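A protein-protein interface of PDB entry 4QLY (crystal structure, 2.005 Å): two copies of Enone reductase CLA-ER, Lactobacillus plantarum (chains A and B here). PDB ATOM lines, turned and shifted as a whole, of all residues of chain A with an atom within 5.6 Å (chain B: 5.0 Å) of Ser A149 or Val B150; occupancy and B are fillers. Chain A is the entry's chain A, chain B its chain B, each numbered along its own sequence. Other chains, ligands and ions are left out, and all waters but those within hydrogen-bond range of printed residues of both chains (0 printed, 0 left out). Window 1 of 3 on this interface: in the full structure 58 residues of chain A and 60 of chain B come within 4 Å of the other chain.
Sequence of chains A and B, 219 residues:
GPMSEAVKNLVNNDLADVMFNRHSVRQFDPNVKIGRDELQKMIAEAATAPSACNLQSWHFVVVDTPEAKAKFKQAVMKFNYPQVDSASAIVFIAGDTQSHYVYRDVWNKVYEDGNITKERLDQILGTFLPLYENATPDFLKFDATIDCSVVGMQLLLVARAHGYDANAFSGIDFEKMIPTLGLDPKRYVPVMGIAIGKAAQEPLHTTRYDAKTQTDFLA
Of the 13 printed residues of chain A, 8 touch a printed residue of chain B.
Printed residues of chain A that touch a printed residue of chain B: Thr A145, Ile A146, Ser A149, Val A150, Met A153, Gln A154, Val A191 and Met A192.
Of the 12 printed residues of chain B, 6 touch a printed residue of chain A.
Along chain B the printed residues that touch a printed residue of chain A span positions 50 to 154.
Among the printed residues, no Asp or Glu carboxylate lies within 4 Å of a Lys or Arg side-chain nitrogen of the other chain.
O of Thr A145 is in hydrogen-bond range of OG of Ser A149, at 2.8 Å.
The backbone NH (N) of Ala B49 lies close to the side-chain amide nitrogen (NE2) of Gln B154, 3.3 Å away.
Printed residues of chain B within 4 Å of Val A150: Ser B149 and Met B153.
Of the printed residues of chain B, Met A153 touches Pro B50, Val B150 and Gln B154.
Of the printed residues of chain B, Val A191 touches Ile B146 (3.97 Å).
Printed residues of chain B within 4 Å of Met A192: Ile B146 (3.7 Å).
Printed residues of chain A within 4 Å of Pro B50: Met A153.
Of chain A, only Ser A149 and Met A153 come within 4 Å of Val B150.
The nearest printed residue of chain B that does not touch Ser A149 is Met B153 (5.4 Å).
Ile A146 touches Ser B149, and with the chains exchanged Ser A149 touches Ile B146.
Ser A149 touches its own counterpart, Ser B149.
Ser A149 touches Val B150, and with the chains exchanged Val A150 touches Ser B149.
Val A150 touches Met B153, and with the chains exchanged Met A153 touches Val B150.
9 positions are printed for both chains.
Ile A146 touches Ser B149 (CG1 to OG, 3.5 Å).
CG1 of Ile B146 touches OG of Ser A149 (3.5 Å).
Ser A149 touches Ser B149.
Ser A149 touches Val B150.
Val A150 touches Met B153.
Met A153 touches Pro B50.
O of Val B150 touches CG of Met A153, at 3.6 Å.
CE of Met A153 touches OE1 of Gln B154, at 3.2 Å.
Met B153 touches Gln A154.
CG2 of Ile B146 touches CE of Met A192, at 3.7 Å.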
ATOM      1  N   ALA A 144     -19.736  15.728   5.535  1.00  0.00           N
ATOM      2  CA  ALA A 144     -20.871  16.159   4.716  1.00  0.00           C
ATOM      3  C   ALA A 144     -22.168  16.102   5.519  1.00  0.00           C
ATOM      4  O   ALA A 144     -23.046  16.949   5.369  1.00  0.00           O
ATOM      5  CB  ALA A 144     -20.991  15.299   3.455  1.00  0.00           C
ATOM      6  N   THR A 145     -22.273  15.104   6.386  1.00  0.00           N
ATOM      7  CA  THR A 145     -23.447  14.966   7.257  1.00  0.00           C
ATOM      8  C   THR A 145     -23.598  16.155   8.207  1.00  0.00           C
ATOM      9  O   THR A 145     -24.700  16.676   8.391  1.00  0.00           O
ATOM     10  CB  THR A 145     -23.368  13.646   8.047  1.00  0.00           C
ATOM     11  OG1 THR A 145     -23.393  12.558   7.111  1.00  0.00           O
ATOM     12  CG2 THR A 145     -24.534  13.514   9.024  1.00  0.00           C
ATOM     13  N   ILE A 146     -22.490  16.607   8.788  1.00  0.00           N
ATOM     14  CA  ILE A 146     -22.523  17.773   9.665  1.00  0.00           C
ATOM     15  C   ILE A 146     -22.996  19.001   8.894  1.00  0.00           C
ATOM     16  O   ILE A 146     -23.896  19.719   9.337  1.00  0.00           O
ATOM     17  CB  ILE A 146     -21.125  18.040  10.302  1.00  0.00           C
ATOM     18  CG1 ILE A 146     -20.733  16.891  11.231  1.00  0.00           C
ATOM     19  CG2 ILE A 146     -21.111  19.366  11.054  1.00  0.00           C
ATOM     20  CD1 ILE A 146     -19.272  16.971  11.714  1.00  0.00           C
ATOM     21  N   ASP A 147     -22.404  19.225   7.718  1.00  0.00           N
ATOM     22  CA  ASP A 147     -22.807  20.334   6.865  1.00  0.00           C
ATOM     23  C   ASP A 147     -24.307  20.267   6.547  1.00  0.00           C
ATOM     24  O   ASP A 147     -25.026  21.251   6.678  1.00  0.00           O
ATOM     25  CB  ASP A 147     -21.996  20.341   5.560  1.00  0.00           C
ATOM     26  CG  ASP A 147     -20.525  20.661   5.763  1.00  0.00           C
ATOM     27  OD1 ASP A 147     -20.112  20.988   6.899  1.00  0.00           O
ATOM     28  OD2 ASP A 147     -19.770  20.612   4.750  1.00  0.00           O
ATOM     29  N   CYS A 148     -24.780  19.104   6.123  1.00  0.00           N
ATOM     30  CA  CYS A 148     -26.205  18.932   5.836  1.00  0.00           C
ATOM     31  C   CYS A 148     -27.094  19.222   7.034  1.00  0.00           C
ATOM     32  O   CYS A 148     -28.186  19.783   6.900  1.00  0.00           O
ATOM     33  CB  CYS A 148     -26.477  17.514   5.342  1.00  0.00           C
ATOM     34  SG  CYS A 148     -25.904  17.287   3.663  1.00  0.00           S
ATOM     35  N   SER A 149     -26.613  18.855   8.207  1.00  0.00           N
ATOM     36  CA  SER A 149     -27.403  19.038   9.422  1.00  0.00           C
ATOM     37  C   SER A 149     -27.465  20.500   9.864  1.00  0.00           C
ATOM     38  O   SER A 149     -28.530  20.974  10.238  1.00  0.00           O
ATOM     39  CB  SER A 149     -26.839  18.184  10.544  1.00  0.00           C
ATOM     40  OG  SER A 149     -26.811  16.817  10.161  1.00  0.00           O
ATOM     41  N   VAL A 150     -26.337  21.213   9.829  1.00  0.00           N
ATOM     42  CA  VAL A 150     -26.372  22.603  10.261  1.00  0.00           C
ATOM     43  C   VAL A 150     -27.211  23.443   9.288  1.00  0.00           C
ATOM     44  O   VAL A 150     -27.974  24.300   9.727  1.00  0.00           O
ATOM     45  CB  VAL A 150     -24.959  23.206  10.430  1.00  0.00           C
ATOM     46  CG1 VAL A 150     -24.187  22.470  11.552  1.00  0.00           C
ATOM     47  CG2 VAL A 150     -24.163  23.194   9.108  1.00  0.00           C
ATOM     48  N   VAL A 151     -27.102  23.195   7.979  1.00  0.00           N
ATOM     49  CA  VAL A 151     -27.937  23.933   7.041  1.00  0.00           C
ATOM     50  C   VAL A 151     -29.410  23.496   7.165  1.00  0.00           C
ATOM     51  O   VAL A 151     -30.321  24.321   7.039  1.00  0.00           O
ATOM     52  CB  VAL A 151     -27.427  23.790   5.562  1.00  0.00           C
ATOM     53  CG1 VAL A 151     -27.755  22.427   4.966  1.00  0.00           C
ATOM     54  CG2 VAL A 151     -27.985  24.909   4.708  1.00  0.00           C
ATOM     55  N   GLY A 152     -29.650  22.217   7.441  1.00  0.00           N
ATOM     56  CA  GLY A 152     -31.002  21.754   7.724  1.00  0.00           C
ATOM     57  C   GLY A 152     -31.609  22.459   8.932  1.00  0.00           C
ATOM     58  O   GLY A 152     -32.762  22.900   8.910  1.00  0.00           O
ATOM     59  N   MET A 153     -30.817  22.585   9.988  1.00  0.00           N
ATOM     60  CA  MET A 153     -31.268  23.307  11.171  1.00  0.00           C
ATOM     61  C   MET A 153     -31.604  24.762  10.823  1.00  0.00           C
ATOM     62  O   MET A 153     -32.608  25.301  11.273  1.00  0.00           O
ATOM     63  CB  MET A 153     -30.204  23.256  12.273  1.00  0.00           C
ATOM     64  CG  MET A 153     -30.641  23.904  13.585  1.00  0.00           C
ATOM     65  SD  MET A 153     -31.972  22.971  14.410  1.00  0.00           S
ATOM     66  CE  MET A 153     -33.336  24.099  14.197  1.00  0.00           C
ATOM     67  N   GLN A 154     -30.773  25.403  10.017  1.00  0.00           N
ATOM     68  CA  GLN A 154     -31.077  26.785   9.666  1.00  0.00           C
ATOM     69  C   GLN A 154     -32.338  26.857   8.790  1.00  0.00           C
ATOM     70  O   GLN A 154     -33.136  27.783   8.919  1.00  0.00           O
ATOM     71  CB  GLN A 154     -29.886  27.447   8.973  1.00  0.00           C
ATOM     72  CG  GLN A 154     -28.744  27.720   9.943  1.00  0.00           C
ATOM     73  CD  GLN A 154     -28.053  29.046   9.683  1.00  0.00           C
ATOM     74  OE1 GLN A 154     -27.666  29.740  10.614  1.00  0.00           O
ATOM     75  NE2 GLN A 154     -27.897  29.405   8.413  1.00  0.00           N
ATOM     76  N   VAL A 191     -29.329  12.463   4.029  1.00  0.00           N
ATOM     77  CA  VAL A 191     -29.256  12.880   5.418  1.00  0.00           C
ATOM     78  C   VAL A 191     -30.633  13.122   6.018  1.00  0.00           C
ATOM     79  O   VAL A 191     -31.029  12.411   6.938  1.00  0.00           O
ATOM     80  CB  VAL A 191     -28.389  14.135   5.590  1.00  0.00           C
ATOM     81  CG1 VAL A 191     -28.438  14.600   7.035  1.00  0.00           C
ATOM     82  CG2 VAL A 191     -26.949  13.828   5.191  1.00  0.00           C
ATOM     83  N   MET A 192     -31.367  14.110   5.521  1.00  0.00           N
ATOM     84  CA  MET A 192     -32.708  14.349   6.050  1.00  0.00           C
ATOM     85  C   MET A 192     -33.605  15.062   5.058  1.00  0.00           C
ATOM     86  O   MET A 192     -33.121  15.755   4.141  1.00  0.00           O
ATOM     87  CB  MET A 192     -32.642  15.169   7.346  1.00  0.00           C
ATOM     88  CG  MET A 192     -32.274  16.616   7.127  1.00  0.00           C
ATOM     89  SD  MET A 192     -32.081  17.573   8.642  1.00  0.00           S
ATOM     90  CE  MET A 192     -30.619  16.851   9.373  1.00  0.00           C
ATOM     91  N   ALA B  49     -33.327  22.366  20.107  1.00  0.00           N
ATOM     92  CA  ALA B  49     -33.127  21.757  18.797  1.00  0.00           C
ATOM     93  C   ALA B  49     -33.886  20.444  18.671  1.00  0.00           C
ATOM     94  O   ALA B  49     -34.137  19.774  19.687  1.00  0.00           O
ATOM     95  CB  ALA B  49     -31.627  21.534  18.545  1.00  0.00           C
ATOM     96  N   PRO B  50     -34.267  20.081  17.431  1.00  0.00           N
ATOM     97  CA  PRO B  50     -34.905  18.787  17.173  1.00  0.00           C
ATOM     98  C   PRO B  50     -33.895  17.649  17.211  1.00  0.00           C
ATOM     99  O   PRO B  50     -32.684  17.892  17.225  1.00  0.00           O
ATOM    100  CB  PRO B  50     -35.485  18.954  15.763  1.00  0.00           C
ATOM    101  CG  PRO B  50     -34.560  19.928  15.093  1.00  0.00           C
ATOM    102  CD  PRO B  50     -34.035  20.840  16.180  1.00  0.00           C
ATOM    103  N   TRP B  58     -26.992  14.641  22.324  1.00  0.00           N
ATOM    104  CA  TRP B  58     -25.817  15.504  22.481  1.00  0.00           C
ATOM    105  C   TRP B  58     -25.280  15.432  23.910  1.00  0.00           C
ATOM    106  O   TRP B  58     -26.045  15.189  24.843  1.00  0.00           O
ATOM    107  CB  TRP B  58     -26.169  16.951  22.125  1.00  0.00           C
ATOM    108  CG  TRP B  58     -27.573  17.350  22.563  1.00  0.00           C
ATOM    109  CD1 TRP B  58     -28.018  17.564  23.839  1.00  0.00           C
ATOM    110  CD2 TRP B  58     -28.697  17.569  21.708  1.00  0.00           C
ATOM    111  NE1 TRP B  58     -29.341  17.920  23.830  1.00  0.00           N
ATOM    112  CE2 TRP B  58     -29.785  17.927  22.529  1.00  0.00           C
ATOM    113  CE3 TRP B  58     -28.884  17.508  20.318  1.00  0.00           C
ATOM    114  CZ2 TRP B  58     -31.052  18.214  22.011  1.00  0.00           C
ATOM    115  CZ3 TRP B  58     -30.140  17.795  19.801  1.00  0.00           C
ATOM    116  CH2 TRP B  58     -31.205  18.148  20.644  1.00  0.00           C
ATOM    117  N   ILE B 146     -25.690  13.970  13.709  1.00  0.00           N
ATOM    118  CA  ILE B 146     -26.730  14.885  13.246  1.00  0.00           C
ATOM    119  C   ILE B 146     -27.290  15.690  14.403  1.00  0.00           C
ATOM    120  O   ILE B 146     -27.435  16.909  14.316  1.00  0.00           O
ATOM    121  CB  ILE B 146     -27.893  14.134  12.533  1.00  0.00           C
ATOM    122  CG1 ILE B 146     -27.414  13.528  11.211  1.00  0.00           C
ATOM    123  CG2 ILE B 146     -29.044  15.071  12.271  1.00  0.00           C
ATOM    124  CD1 ILE B 146     -28.481  12.670  10.508  1.00  0.00           C
ATOM    125  N   ASP B 147     -27.609  14.998  15.493  1.00  0.00           N
ATOM    126  CA  ASP B 147     -28.092  15.655  16.686  1.00  0.00           C
ATOM    127  C   ASP B 147     -27.087  16.691  17.198  1.00  0.00           C
ATOM    128  O   ASP B 147     -27.446  17.826  17.494  1.00  0.00           O
ATOM    129  CB  ASP B 147     -28.367  14.621  17.777  1.00  0.00           C
ATOM    130  CG  ASP B 147     -29.667  13.874  17.567  1.00  0.00           C
ATOM    131  OD1 ASP B 147     -30.357  14.111  16.541  1.00  0.00           O
ATOM    132  OD2 ASP B 147     -29.989  13.048  18.452  1.00  0.00           O
ATOM    133  N   CYS B 148     -25.832  16.287  17.315  1.00  0.00           N
ATOM    134  CA  CYS B 148     -24.788  17.194  17.764  1.00  0.00           C
ATOM    135  C   CYS B 148     -24.668  18.413  16.856  1.00  0.00           C
ATOM    136  O   CYS B 148     -24.420  19.535  17.310  1.00  0.00           O
ATOM    137  CB  CYS B 148     -23.455  16.453  17.826  1.00  0.00           C
ATOM    138  SG  CYS B 148     -23.416  15.315  19.225  1.00  0.00           S
ATOM    139  N   SER B 149     -24.876  18.188  15.568  1.00  0.00           N
ATOM    140  CA  SER B 149     -24.719  19.262  14.587  1.00  0.00           C
ATOM    141  C   SER B 149     -25.851  20.288  14.652  1.00  0.00           C
ATOM    142  O   SER B 149     -25.590  21.491  14.592  1.00  0.00           O
ATOM    143  CB  SER B 149     -24.620  18.676  13.187  1.00  0.00           C
ATOM    144  OG  SER B 149     -23.521  17.793  13.111  1.00  0.00           O
ATOM    145  N   VAL B 150     -27.095  19.830  14.800  1.00  0.00           N
ATOM    146  CA  VAL B 150     -28.200  20.782  14.835  1.00  0.00           C
ATOM    147  C   VAL B 150     -28.175  21.569  16.150  1.00  0.00           C
ATOM    148  O   VAL B 150     -28.471  22.766  16.160  1.00  0.00           O
ATOM    149  CB  VAL B 150     -29.604  20.095  14.611  1.00  0.00           C
ATOM    150  CG1 VAL B 150     -29.676  19.440  13.213  1.00  0.00           C
ATOM    151  CG2 VAL B 150     -29.959  19.092  15.720  1.00  0.00           C
ATOM    152  N   VAL B 151     -27.793  20.932  17.264  1.00  0.00           N
ATOM    153  CA  VAL B 151     -27.721  21.692  18.507  1.00  0.00           C
ATOM    154  C   VAL B 151     -26.483  22.613  18.443  1.00  0.00           C
ATOM    155  O   VAL B 151     -26.506  23.753  18.930  1.00  0.00           O
ATOM    156  CB  VAL B 151     -27.694  20.766  19.780  1.00  0.00           C
ATOM    157  CG1 VAL B 151     -26.317  20.134  20.024  1.00  0.00           C
ATOM    158  CG2 VAL B 151     -28.120  21.559  20.993  1.00  0.00           C
ATOM    159  N   GLY B 152     -25.413  22.115  17.828  1.00  0.00           N
ATOM    160  CA  GLY B 152     -24.238  22.938  17.565  1.00  0.00           C
ATOM    161  C   GLY B 152     -24.629  24.194  16.803  1.00  0.00           C
ATOM    162  O   GLY B 152     -24.228  25.296  17.189  1.00  0.00           O
ATOM    163  N   MET B 153     -25.439  24.030  15.748  1.00  0.00           N
ATOM    164  CA  MET B 153     -25.837  25.177  14.926  1.00  0.00           C
ATOM    165  C   MET B 153     -26.644  26.160  15.763  1.00  0.00           C
ATOM    166  O   MET B 153     -26.465  27.375  15.642  1.00  0.00           O
ATOM    167  CB  MET B 153     -26.660  24.747  13.697  1.00  0.00           C
ATOM    168  CG  MET B 153     -27.044  25.928  12.757  1.00  0.00           C
ATOM    169  SD  MET B 153     -25.639  26.669  11.866  1.00  0.00           S
ATOM    170  CE  MET B 153     -25.579  28.339  12.536  1.00  0.00           C
ATOM    171  N   GLN B 154     -27.540  25.641  16.606  1.00  0.00           N
ATOM    172  CA  GLN B 154     -28.348  26.526  17.423  1.00  0.00           C
ATOM    173  C   GLN B 154     -27.476  27.228  18.473  1.00  0.00           C
ATOM    174  O   GLN B 154     -27.671  28.418  18.746  1.00  0.00           O
ATOM    175  CB  GLN B 154     -29.511  25.761  18.076  1.00  0.00           C
ATOM    176  CG  GLN B 154     -30.585  25.349  17.063  1.00  0.00           C
ATOM    177  CD  GLN B 154     -32.017  25.477  17.587  1.00  0.00           C
ATOM    178  OE1 GLN B 154     -32.935  25.824  16.839  1.00  0.00           O
ATOM    179  NE2 GLN B 154     -32.215  25.169  18.869  1.00  0.00           N
